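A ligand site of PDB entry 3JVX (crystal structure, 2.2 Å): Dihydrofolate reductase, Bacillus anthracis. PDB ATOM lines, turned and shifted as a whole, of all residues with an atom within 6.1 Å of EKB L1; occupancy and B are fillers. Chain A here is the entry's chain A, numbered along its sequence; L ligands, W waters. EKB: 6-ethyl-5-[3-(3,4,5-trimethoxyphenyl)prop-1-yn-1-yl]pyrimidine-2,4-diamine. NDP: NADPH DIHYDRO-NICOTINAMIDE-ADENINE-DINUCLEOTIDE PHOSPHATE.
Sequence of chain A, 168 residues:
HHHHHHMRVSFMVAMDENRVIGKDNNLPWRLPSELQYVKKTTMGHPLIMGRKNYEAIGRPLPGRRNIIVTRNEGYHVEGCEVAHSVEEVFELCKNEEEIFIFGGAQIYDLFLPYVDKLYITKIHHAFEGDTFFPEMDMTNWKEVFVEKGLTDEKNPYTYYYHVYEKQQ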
ATOM      1  N   MET A  12      -7.106   9.069  -0.822  1.00  0.00           N
ATOM      2  CA  MET A  12      -6.016   9.440  -1.706  1.00  0.00           C
ATOM      3  C   MET A  12      -5.904   8.368  -2.808  1.00  0.00           C
ATOM      4  O   MET A  12      -5.621   7.211  -2.505  1.00  0.00           O
ATOM      5  CB  MET A  12      -4.710   9.600  -0.921  1.00  0.00           C
ATOM      6  CG  MET A  12      -3.441   9.794  -1.763  1.00  0.00           C
ATOM      7  SD  MET A  12      -3.386  11.279  -2.789  1.00  0.00           S
ATOM      8  CE  MET A  12      -3.352  12.588  -1.555  1.00  0.00           C
ATOM      9  N   VAL A  13      -6.138   8.780  -4.055  1.00  0.00           N
ATOM     10  CA  VAL A  13      -6.201   7.845  -5.189  1.00  0.00           C
ATOM     11  C   VAL A  13      -5.773   8.475  -6.530  1.00  0.00           C
ATOM     12  O   VAL A  13      -5.946   9.669  -6.752  1.00  0.00           O
ATOM     13  CB  VAL A  13      -7.624   7.185  -5.289  1.00  0.00           C
ATOM     14  CG1 VAL A  13      -8.699   8.216  -5.651  1.00  0.00           C
ATOM     15  CG2 VAL A  13      -7.632   5.991  -6.257  1.00  0.00           C
ATOM     16  N   ALA A  14      -5.159   7.666  -7.389  1.00  0.00           N
ATOM     17  CA  ALA A  14      -4.897   8.042  -8.784  1.00  0.00           C
ATOM     18  C   ALA A  14      -5.568   6.999  -9.690  1.00  0.00           C
ATOM     19  O   ALA A  14      -5.356   5.782  -9.533  1.00  0.00           O
ATOM     20  CB  ALA A  14      -3.409   8.119  -9.057  1.00  0.00           C
ATOM     21  N   ASN A  25      -1.867  -6.751  -9.564  1.00  0.00           N
ATOM     22  CA  ASN A  25      -1.440  -6.388  -8.203  1.00  0.00           C
ATOM     23  C   ASN A  25      -0.346  -5.304  -8.133  1.00  0.00           C
ATOM     24  O   ASN A  25       0.434  -5.256  -7.179  1.00  0.00           O
ATOM     25  CB  ASN A  25      -1.024  -7.650  -7.417  1.00  0.00           C
ATOM     26  CG  ASN A  25      -1.211  -7.516  -5.911  1.00  0.00           C
ATOM     27  OD1 ASN A  25      -2.120  -6.823  -5.433  1.00  0.00           O
ATOM     28  ND2 ASN A  25      -0.350  -8.198  -5.158  1.00  0.00           N
ATOM     29  N   ASN A  26      -0.298  -4.439  -9.148  1.00  0.00           N
ATOM     30  CA  ASN A  26       0.668  -3.322  -9.207  1.00  0.00           C
ATOM     31  C   ASN A  26       0.015  -2.107  -9.871  1.00  0.00           C
ATOM     32  O   ASN A  26      -1.153  -2.164 -10.286  1.00  0.00           O
ATOM     33  CB  ASN A  26       1.931  -3.748  -9.988  1.00  0.00           C
ATOM     34  CG  ASN A  26       3.205  -2.945  -9.593  1.00  0.00           C
ATOM     35  OD1 ASN A  26       3.141  -1.895  -8.934  1.00  0.00           O
ATOM     36  ND2 ASN A  26       4.363  -3.457 -10.016  1.00  0.00           N
ATOM     37  N   LEU A  27       0.778  -1.012  -9.969  1.00  0.00           N
ATOM     38  CA  LEU A  27       0.334   0.214 -10.637  1.00  0.00           C
ATOM     39  C   LEU A  27       0.537   0.109 -12.142  1.00  0.00           C
ATOM     40  O   LEU A  27       1.587  -0.359 -12.597  1.00  0.00           O
ATOM     41  CB  LEU A  27       1.101   1.423 -10.107  1.00  0.00           C
ATOM     42  CG  LEU A  27       1.028   1.723  -8.595  1.00  0.00           C
ATOM     43  CD1 LEU A  27       1.983   2.860  -8.226  1.00  0.00           C
ATOM     44  CD2 LEU A  27      -0.417   2.058  -8.177  1.00  0.00           C
ATOM     45  N   TRP A  29       0.983   2.543 -14.244  1.00  0.00           N
ATOM     46  CA  TRP A  29       1.779   3.656 -14.760  1.00  0.00           C
ATOM     47  C   TRP A  29       2.900   4.039 -13.790  1.00  0.00           C
ATOM     48  O   TRP A  29       2.858   3.679 -12.603  1.00  0.00           O
ATOM     49  CB  TRP A  29       0.882   4.883 -14.977  1.00  0.00           C
ATOM     50  CG  TRP A  29       0.109   5.237 -13.736  1.00  0.00           C
ATOM     51  CD1 TRP A  29       0.578   5.923 -12.650  1.00  0.00           C
ATOM     52  CD2 TRP A  29      -1.257   4.905 -13.443  1.00  0.00           C
ATOM     53  NE1 TRP A  29      -0.414   6.050 -11.710  1.00  0.00           N
ATOM     54  CE2 TRP A  29      -1.549   5.429 -12.166  1.00  0.00           C
ATOM     55  CE3 TRP A  29      -2.262   4.233 -14.142  1.00  0.00           C
ATOM     56  CZ2 TRP A  29      -2.805   5.289 -11.567  1.00  0.00           C
ATOM     57  CZ3 TRP A  29      -3.518   4.083 -13.543  1.00  0.00           C
ATOM     58  CH2 TRP A  29      -3.768   4.605 -12.259  1.00  0.00           C
ATOM     59  N   GLU A  34       3.780  12.611  -9.550  1.00  0.00           N
ATOM     60  CA  GLU A  34       2.503  12.343  -8.900  1.00  0.00           C
ATOM     61  C   GLU A  34       2.740  11.714  -7.510  1.00  0.00           C
ATOM     62  O   GLU A  34       2.019  12.039  -6.554  1.00  0.00           O
ATOM     63  CB  GLU A  34       1.660  11.419  -9.780  1.00  0.00           C
ATOM     64  CG  GLU A  34       0.148  11.561  -9.611  1.00  0.00           C
ATOM     65  CD  GLU A  34      -0.381  10.832  -8.384  1.00  0.00           C
ATOM     66  OE1 GLU A  34       0.081   9.707  -8.111  1.00  0.00           O
ATOM     67  OE2 GLU A  34      -1.260  11.389  -7.682  1.00  0.00           O
ATOM     68  N   LEU A  35       3.734  10.831  -7.410  1.00  0.00           N
ATOM     69  CA  LEU A  35       4.135  10.262  -6.125  1.00  0.00           C
ATOM     70  C   LEU A  35       4.661  11.313  -5.163  1.00  0.00           C
ATOM     71  O   LEU A  35       4.427  11.221  -3.959  1.00  0.00           O
ATOM     72  CB  LEU A  35       5.186   9.169  -6.303  1.00  0.00           C
ATOM     73  CG  LEU A  35       4.662   7.739  -6.393  1.00  0.00           C
ATOM     74  CD1 LEU A  35       4.025   7.495  -7.748  1.00  0.00           C
ATOM     75  CD2 LEU A  35       5.787   6.743  -6.154  1.00  0.00           C
ATOM     76  N   TYR A  37       3.715  14.460  -5.118  1.00  0.00           N
ATOM     77  CA  TYR A  37       2.477  15.097  -4.662  1.00  0.00           C
ATOM     78  C   TYR A  37       1.779  14.293  -3.559  1.00  0.00           C
ATOM     79  O   TYR A  37       1.295  14.869  -2.587  1.00  0.00           O
ATOM     80  CB  TYR A  37       1.522  15.292  -5.845  1.00  0.00           C
ATOM     81  CG  TYR A  37       0.112  15.706  -5.439  1.00  0.00           C
ATOM     82  CD1 TYR A  37      -0.881  14.745  -5.174  1.00  0.00           C
ATOM     83  CD2 TYR A  37      -0.223  17.055  -5.333  1.00  0.00           C
ATOM     84  CE1 TYR A  37      -2.158  15.122  -4.802  1.00  0.00           C
ATOM     85  CE2 TYR A  37      -1.508  17.442  -4.956  1.00  0.00           C
ATOM     86  CZ  TYR A  37      -2.485  16.460  -4.702  1.00  0.00           C
ATOM     87  OH  TYR A  37      -3.760  16.837  -4.345  1.00  0.00           O
ATOM     88  N   VAL A  38       1.738  12.980  -3.726  1.00  0.00           N
ATOM     89  CA  VAL A  38       1.181  12.067  -2.727  1.00  0.00           C
ATOM     90  C   VAL A  38       1.936  12.114  -1.397  1.00  0.00           C
ATOM     91  O   VAL A  38       1.312  12.237  -0.340  1.00  0.00           O
ATOM     92  CB  VAL A  38       1.127  10.595  -3.256  1.00  0.00           C
ATOM     93  CG1 VAL A  38       0.683   9.649  -2.166  1.00  0.00           C
ATOM     94  CG2 VAL A  38       0.205  10.498  -4.454  1.00  0.00           C
ATOM     95  N   ASN A  53      -2.392  -3.996  -1.114  1.00  0.00           N
ATOM     96  CA  ASN A  53      -1.706  -2.741  -1.401  1.00  0.00           C
ATOM     97  C   ASN A  53      -0.389  -2.662  -0.613  1.00  0.00           C
ATOM     98  O   ASN A  53       0.666  -2.442  -1.189  1.00  0.00           O
ATOM     99  CB  ASN A  53      -2.609  -1.542  -1.095  1.00  0.00           C
ATOM    100  CG  ASN A  53      -1.945  -0.197  -1.403  1.00  0.00           C
ATOM    101  OD1 ASN A  53      -1.114  -0.096  -2.312  1.00  0.00           O
ATOM    102  ND2 ASN A  53      -2.318   0.828  -0.656  1.00  0.00           N
ATOM    103  N   ALA A  56       2.556  -5.106  -1.851  1.00  0.00           N
ATOM    104  CA  ALA A  56       3.156  -4.632  -3.095  1.00  0.00           C
ATOM    105  C   ALA A  56       4.151  -3.489  -2.841  1.00  0.00           C
ATOM    106  O   ALA A  56       5.214  -3.431  -3.461  1.00  0.00           O
ATOM    107  CB  ALA A  56       2.076  -4.216  -4.075  1.00  0.00           C
ATOM    108  N   ILE A  57       3.811  -2.581  -1.921  1.00  0.00           N
ATOM    109  CA  ILE A  57       4.726  -1.511  -1.499  1.00  0.00           C
ATOM    110  C   ILE A  57       5.949  -2.120  -0.798  1.00  0.00           C
ATOM    111  O   ILE A  57       7.086  -1.778  -1.135  1.00  0.00           O
ATOM    112  CB  ILE A  57       4.023  -0.467  -0.612  1.00  0.00           C
ATOM    113  CG1 ILE A  57       2.892   0.217  -1.380  1.00  0.00           C
ATOM    114  CG2 ILE A  57       5.041   0.571  -0.080  1.00  0.00           C
ATOM    115  CD1 ILE A  57       1.933   1.001  -0.519  1.00  0.00           C
ATOM    116  N   ARG A  59       7.286  -2.008   2.235  1.00  0.00           N
ATOM    117  CA  ARG A  59       8.035  -1.316   3.280  1.00  0.00           C
ATOM    118  C   ARG A  59       7.151  -0.231   3.879  1.00  0.00           C
ATOM    119  O   ARG A  59       6.312   0.341   3.182  1.00  0.00           O
ATOM    120  CB  ARG A  59       9.308  -0.696   2.698  1.00  0.00           C
ATOM    121  CG  ARG A  59       9.016   0.179   1.485  1.00  0.00           C
ATOM    122  CD  ARG A  59      10.229   0.861   0.849  1.00  0.00           C
ATOM    123  NE  ARG A  59       9.777   1.594  -0.335  1.00  0.00           N
ATOM    124  CZ  ARG A  59       9.293   2.838  -0.308  1.00  0.00           C
ATOM    125  NH1 ARG A  59       9.214   3.510   0.841  1.00  0.00           N
ATOM    126  NH2 ARG A  59       8.904   3.420  -1.441  1.00  0.00           N
ATOM    127  N   LEU A  61       6.057   3.303   4.763  1.00  0.00           N
ATOM    128  CA  LEU A  61       6.308   4.599   4.161  1.00  0.00           C
ATOM    129  C   LEU A  61       6.649   5.602   5.281  1.00  0.00           C
ATOM    130  O   LEU A  61       5.891   5.738   6.238  1.00  0.00           O
ATOM    131  CB  LEU A  61       5.108   5.054   3.318  1.00  0.00           C
ATOM    132  CG  LEU A  61       4.757   4.121   2.144  1.00  0.00           C
ATOM    133  CD1 LEU A  61       3.469   4.523   1.474  1.00  0.00           C
ATOM    134  CD2 LEU A  61       5.872   4.017   1.115  1.00  0.00           C
ATOM    135  N   ILE A 101      -7.119   7.195   3.317  1.00  0.00           N
ATOM    136  CA  ILE A 101      -7.418   5.884   2.793  1.00  0.00           C
ATOM    137  C   ILE A 101      -6.637   5.819   1.487  1.00  0.00           C
ATOM    138  O   ILE A 101      -6.885   6.619   0.563  1.00  0.00           O
ATOM    139  CB  ILE A 101      -8.944   5.668   2.599  1.00  0.00           C
ATOM    140  CG1 ILE A 101      -9.749   6.114   3.839  1.00  0.00           C
ATOM    141  CG2 ILE A 101      -9.259   4.211   2.221  1.00  0.00           C
ATOM    142  CD1 ILE A 101      -9.400   5.409   5.185  1.00  0.00           C
ATOM    143  N   PHE A 102      -5.700   4.894   1.444  1.00  0.00           N
ATOM    144  CA  PHE A 102      -4.645   4.854   0.446  1.00  0.00           C
ATOM    145  C   PHE A 102      -4.805   3.686  -0.547  1.00  0.00           C
ATOM    146  O   PHE A 102      -3.934   3.457  -1.389  1.00  0.00           O
ATOM    147  CB  PHE A 102      -3.309   4.721   1.194  1.00  0.00           C
ATOM    148  CG  PHE A 102      -2.112   5.220   0.431  1.00  0.00           C
ATOM    149  CD1 PHE A 102      -2.037   6.548  -0.006  1.00  0.00           C
ATOM    150  CD2 PHE A 102      -1.034   4.365   0.200  1.00  0.00           C
ATOM    151  CE1 PHE A 102      -0.916   7.012  -0.701  1.00  0.00           C
ATOM    152  CE2 PHE A 102       0.093   4.809  -0.500  1.00  0.00           C
ATOM    153  CZ  PHE A 102       0.162   6.137  -0.945  1.00  0.00           C
ATOM    154  N   GLY A 103      -5.915   2.957  -0.430  1.00  0.00           N
ATOM    155  CA  GLY A 103      -6.195   1.837  -1.336  1.00  0.00           C
ATOM    156  C   GLY A 103      -5.815   0.461  -0.796  1.00  0.00           C
ATOM    157  O   GLY A 103      -5.342   0.346   0.329  1.00  0.00           O
ATOM    158  N   TYR A 108     -10.972   0.911  -0.445  1.00  0.00           N
ATOM    159  CA  TYR A 108     -11.788   2.049  -0.869  1.00  0.00           C
ATOM    160  C   TYR A 108     -13.285   1.759  -0.727  1.00  0.00           C
ATOM    161  O   TYR A 108     -14.034   2.625  -0.264  1.00  0.00           O
ATOM    162  CB  TYR A 108     -11.501   2.473  -2.319  1.00  0.00           C
ATOM    163  CG  TYR A 108     -10.155   3.128  -2.546  1.00  0.00           C
ATOM    164  CD1 TYR A 108      -9.712   4.169  -1.734  1.00  0.00           C
ATOM    165  CD2 TYR A 108      -9.360   2.747  -3.618  1.00  0.00           C
ATOM    166  CE1 TYR A 108      -8.491   4.759  -1.958  1.00  0.00           C
ATOM    167  CE2 TYR A 108      -8.136   3.337  -3.856  1.00  0.00           C
ATOM    168  CZ  TYR A 108      -7.713   4.349  -3.017  1.00  0.00           C
ATOM    169  OH  TYR A 108      -6.497   4.940  -3.249  1.00  0.00           O
ATOM    170  N   TYR A 119      -9.003  13.309  -2.560  1.00  0.00           N
ATOM    171  CA  TYR A 119      -7.849  13.780  -3.328  1.00  0.00           C
ATOM    172  C   TYR A 119      -7.637  12.783  -4.453  1.00  0.00           C
ATOM    173  O   TYR A 119      -7.076  11.691  -4.251  1.00  0.00           O
ATOM    174  CB  TYR A 119      -6.586  13.833  -2.476  1.00  0.00           C
ATOM    175  CG  TYR A 119      -6.615  14.744  -1.262  1.00  0.00           C
ATOM    176  CD1 TYR A 119      -7.377  14.415  -0.135  1.00  0.00           C
ATOM    177  CD2 TYR A 119      -5.836  15.902  -1.223  1.00  0.00           C
ATOM    178  CE1 TYR A 119      -7.381  15.232   0.986  1.00  0.00           C
ATOM    179  CE2 TYR A 119      -5.845  16.729  -0.111  1.00  0.00           C
ATOM    180  CZ  TYR A 119      -6.609  16.379   0.981  1.00  0.00           C
ATOM    181  OH  TYR A 119      -6.616  17.196   2.080  1.00  0.00           O
ATOM    182  N   ILE A 120      -8.112  13.147  -5.636  1.00  0.00           N
ATOM    183  CA  ILE A 120      -8.110  12.239  -6.769  1.00  0.00           C
ATOM    184  C   ILE A 120      -7.323  12.796  -7.950  1.00  0.00           C
ATOM    185  O   ILE A 120      -7.617  13.858  -8.481  1.00  0.00           O
ATOM    186  CB  ILE A 120      -9.544  11.773  -7.156  1.00  0.00           C
ATOM    187  CG1 ILE A 120      -9.503  10.714  -8.256  1.00  0.00           C
ATOM    188  CG2 ILE A 120     -10.416  12.964  -7.576  1.00  0.00           C
ATOM    189  CD1 ILE A 120     -10.815   9.930  -8.363  1.00  0.00           C
ATOM    190  N   THR A 121      -6.294  12.050  -8.343  1.00  0.00           N
ATOM    191  CA  THR A 121      -5.549  12.379  -9.545  1.00  0.00           C
ATOM    192  C   THR A 121      -6.207  11.660 -10.717  1.00  0.00           C
ATOM    193  O   THR A 121      -6.436  10.450 -10.673  1.00  0.00           O
ATOM    194  CB  THR A 121      -4.082  11.976  -9.412  1.00  0.00           C
ATOM    195  OG1 THR A 121      -3.538  12.580  -8.233  1.00  0.00           O
ATOM    196  CG2 THR A 121      -3.291  12.432 -10.646  1.00  0.00           C
HETATM  197  N1  EKB L   1      -2.950   7.942  -4.615  1.00  0.00           N
HETATM  198  C2  EKB L   1      -2.353   8.613  -5.608  1.00  0.00           C
HETATM  199  N3  EKB L   1      -1.314   8.080  -6.278  1.00  0.00           N
HETATM  200  C4  EKB L   1      -0.830   6.874  -5.984  1.00  0.00           C
HETATM  201  C5  EKB L   1      -1.441   6.154  -4.956  1.00  0.00           C
HETATM  202  C6  EKB L   1      -2.512   6.710  -4.264  1.00  0.00           C
HETATM  203  C1A EKB L   1      -0.187   5.695  -8.052  1.00  0.00           C
HETATM  204  C1B EKB L   1       3.255  -0.976  -5.849  1.00  0.00           C
HETATM  205  C1C EKB L   1       4.016   5.201  -2.321  1.00  0.00           C
HETATM  206  C1D EKB L   1       6.067   2.791  -5.923  1.00  0.00           C
HETATM  207  N1E EKB L   1      -2.768   9.815  -5.976  1.00  0.00           N
HETATM  208  N1F EKB L   1      -3.101   6.028  -3.276  1.00  0.00           N
HETATM  209  C1G EKB L   1      -0.533   3.736  -4.314  1.00  0.00           C
HETATM  210  C1H EKB L   1      -0.957   4.849  -4.602  1.00  0.00           C
HETATM  211  C1I EKB L   1       2.115   1.254  -4.746  1.00  0.00           C
HETATM  212  C1J EKB L   1       2.306   3.432  -3.729  1.00  0.00           C
HETATM  213  C1K EKB L   1       0.350   6.371  -6.804  1.00  0.00           C
HETATM  214  C1L EKB L   1      -0.009   2.408  -3.989  1.00  0.00           C
HETATM  215  O1O EKB L   1       4.134   0.115  -5.462  1.00  0.00           O
HETATM  216  O1P EKB L   1       4.483   4.442  -3.455  1.00  0.00           O
HETATM  217  O1Q EKB L   1       5.660   2.280  -4.597  1.00  0.00           O
HETATM  218  C1S EKB L   1       1.516   2.366  -4.166  1.00  0.00           C
HETATM  219  C1V EKB L   1       3.514   1.207  -4.893  1.00  0.00           C
HETATM  220  C1W EKB L   1       3.697   3.396  -3.871  1.00  0.00           C
HETATM  221  C1Y EKB L   1       4.291   2.294  -4.458  1.00  0.00           C
HETATM  222  PA  NDP L   2      -6.535  -4.073  -1.266  1.00  0.00           P
HETATM  223  O1A NDP L   2      -7.831  -3.392  -1.150  1.00  0.00           O
HETATM  224  O2A NDP L   2      -5.377  -3.171  -1.108  1.00  0.00           O
HETATM  225  O5B NDP L   2      -6.408  -5.225  -0.171  1.00  0.00           O
HETATM  226  C5B NDP L   2      -7.346  -6.273  -0.132  1.00  0.00           C
HETATM  227  C4B NDP L   2      -7.130  -6.952   1.199  1.00  0.00           C
HETATM  228  O4B NDP L   2      -7.611  -6.096   2.221  1.00  0.00           O
HETATM  229  C3B NDP L   2      -7.870  -8.267   1.365  1.00  0.00           C
HETATM  230  O3B NDP L   2      -7.160  -9.334   0.780  1.00  0.00           O
HETATM  231  C2B NDP L   2      -7.938  -8.338   2.882  1.00  0.00           C
HETATM  232  O2B NDP L   2      -6.714  -8.771   3.449  1.00  0.00           O
HETATM  233  C1B NDP L   2      -8.141  -6.879   3.263  1.00  0.00           C
HETATM  234  N9A NDP L   2      -9.579  -6.640   3.441  1.00  0.00           N
HETATM  235  C8A NDP L   2     -10.532  -6.459   2.467  1.00  0.00           C
HETATM  236  N7A NDP L   2     -11.721  -6.281   3.081  1.00  0.00           N
HETATM  237  C5A NDP L   2     -11.555  -6.367   4.428  1.00  0.00           C
HETATM  238  C6A NDP L   2     -12.427  -6.273   5.504  1.00  0.00           C
HETATM  239  N6A NDP L   2     -13.733  -6.059   5.302  1.00  0.00           N
HETATM  240  N1A NDP L   2     -11.936  -6.385   6.789  1.00  0.00           N
HETATM  241  C2A NDP L   2     -10.598  -6.590   7.017  1.00  0.00           C
HETATM  242  N3A NDP L   2      -9.740  -6.694   5.939  1.00  0.00           N
HETATM  243  C4A NDP L   2     -10.211  -6.582   4.664  1.00  0.00           C
HETATM  244  O3  NDP L   2      -6.494  -4.978  -2.600  1.00  0.00           O
HETATM  245  PN  NDP L   2      -7.017  -4.749  -4.095  1.00  0.00           P
HETATM  246  O1N NDP L   2      -6.677  -5.964  -4.870  1.00  0.00           O
HETATM  247  O2N NDP L   2      -8.408  -4.244  -4.010  1.00  0.00           O
HETATM  248  O5D NDP L   2      -6.118  -3.500  -4.598  1.00  0.00           O
HETATM  249  C5D NDP L   2      -4.775  -3.719  -4.979  1.00  0.00           C
HETATM  250  C4D NDP L   2      -4.515  -3.052  -6.333  1.00  0.00           C
HETATM  251  O4D NDP L   2      -4.806  -1.666  -6.308  1.00  0.00           O
HETATM  252  C3D NDP L   2      -3.057  -3.167  -6.734  1.00  0.00           C
HETATM  253  O3D NDP L   2      -3.045  -3.311  -8.139  1.00  0.00           O
HETATM  254  C2D NDP L   2      -2.486  -1.821  -6.333  1.00  0.00           C
HETATM  255  O2D NDP L   2      -1.305  -1.531  -7.048  1.00  0.00           O
HETATM  256  C1D NDP L   2      -3.655  -0.916  -6.677  1.00  0.00           C
HETATM  257  N1N NDP L   2      -3.670   0.383  -5.988  1.00  0.00           N
HETATM  258  C2N NDP L   2      -3.656   1.505  -6.765  1.00  0.00           C
HETATM  259  C3N NDP L   2      -3.701   2.753  -6.166  1.00  0.00           C
HETATM  260  C7N NDP L   2      -3.892   3.973  -7.029  1.00  0.00           C
HETATM  261  O7N NDP L   2      -4.298   5.138  -6.392  1.00  0.00           O
HETATM  262  N7N NDP L   2      -3.691   3.923  -8.335  1.00  0.00           N
HETATM  263  C4N NDP L   2      -3.777   2.869  -4.778  1.00  0.00           C
HETATM  264  C5N NDP L   2      -3.794   1.717  -3.986  1.00  0.00           C
HETATM  265  C6N NDP L   2      -3.744   0.479  -4.613  1.00  0.00           C
HETATM  266  P2B NDP L   2      -6.439 -10.274   3.891  1.00  0.00           P
HETATM  267  O1X NDP L   2      -6.466 -11.114   2.644  1.00  0.00           O
HETATM  268  O2X NDP L   2      -5.065 -10.382   4.501  1.00  0.00           O
HETATM  269  O3X NDP L   2      -7.521 -10.734   4.842  1.00  0.00           O
HETATM  270  O   HOH W   1       0.821   7.864 -10.106  1.00  0.00           O
HETATM  271  O   HOH W   2      -4.606  12.717  -5.707  1.00  0.00           O
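N1F of EKB L1 lies close to O7N of NDP L2, 3.5 Å away.
The side-chain carboxylate (OE2) of Glu 34 is in hydrogen-bond range of the side-chain hydroxyl (OG1) of Thr 121, at 2.6 Å. O of Met 12 is in hydrogen-bond range of OH of Tyr 108 (2.5 Å). O of Ile 101 is in hydrogen-bond range of N of Met 12. The side-chain amide nitrogen (ND2) of Asn 53 is in hydrogen-bond range of the backbone carbonyl oxygen (O) of Phe 102. The backbone carbonyl oxygen (O) of Gly 103 sits at hydrogen-bond distance from the side-chain amide nitrogen (ND2) of Asn 53, 3.2 Å away. N of Thr 121 sits at hydrogen-bond distance from O of Val 13, at 2.9 Å. O of Tyr 119 is in hydrogen-bond range of N of Val 13 (3.1 Å). OH of Tyr 108 lies close to O of Phe 102 (3.5 Å).
N of Ala 14 touches C2 of EKB L1, 3.5 Å away. Asn 26 touches EKB L1 (OD1 to C1B, 3.2 Å). Leu 27 touches EKB L1 (CD1 to C1A, 3.6 Å). Trp 29 touches EKB L1. Leu 35 touches EKB L1. Val 38 touches EKB L1. Asn 53 touches EKB L1. Ala 56 touches EKB L1 (CB to C1B, 3.9 Å). CG1 of Ile 57 touches C1I of EKB L1, 3.6 Å away. Leu 61 touches EKB L1. Tyr 108 touches EKB L1. Thr 121 touches EKB L1. Hydrophobic or aromatic side chains that line EKB L1: Met 12, Ala 14, Leu 27, Leu 35, Val 38, Ala 56, Ile 57, Leu 61 and Phe 102. Of the 23 residues printed, 16 come within 4 Å of EKB L1. The nearest printed residue that does not touch EKB L1 is Arg 59 (4.7 Å).
Water W1 bridges the indole nitrogen (NE1) of Trp 29 and the side-chain carboxylate (OE1) of Glu 34.
A nitrogen (N1E) of EKB L1 is in hydrogen-bond range of the side-chain carboxylate of Glu 34 (2.8 Å). N1F of EKB L1 lies within hydrogen-bond range of O of Met 12, at 2.9 Å. SD of Met 12 sits at hydrogen-bond distance from N1E of EKB L1, 3.6 Å away. The backbone NH (N) of Val 13 lies close to a nitrogen (N1) of EKB L1, at 3.3 Å. The backbone carbonyl oxygen of Val 13 is in hydrogen-bond range of a nitrogen (N1E) of EKB L1 (3.3 Å). O of Phe 102 lies within hydrogen-bond range of N1F of EKB L1, 3.3 Å away. The backbone NH (N) of Asn 53 lies within hydrogen-bond range of an oxygen (O2A) of NDP L2. The backbone NH of Asn 26 lies within hydrogen-bond range of an oxygen (O3D) of NDP L2 (3.1 Å). The backbone carbonyl oxygen of Asn 26 is in hydrogen-bond range of an oxygen (O3D) of NDP L2 (3.1 Å). An oxygen (O7N) of NDP L2 is in hydrogen-bond range of the backbone NH (N) of Ala 14, 2.9 Å away. N7N of NDP L2 sits at hydrogen-bond distance from O of Ala 14, 2.8 Å away.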
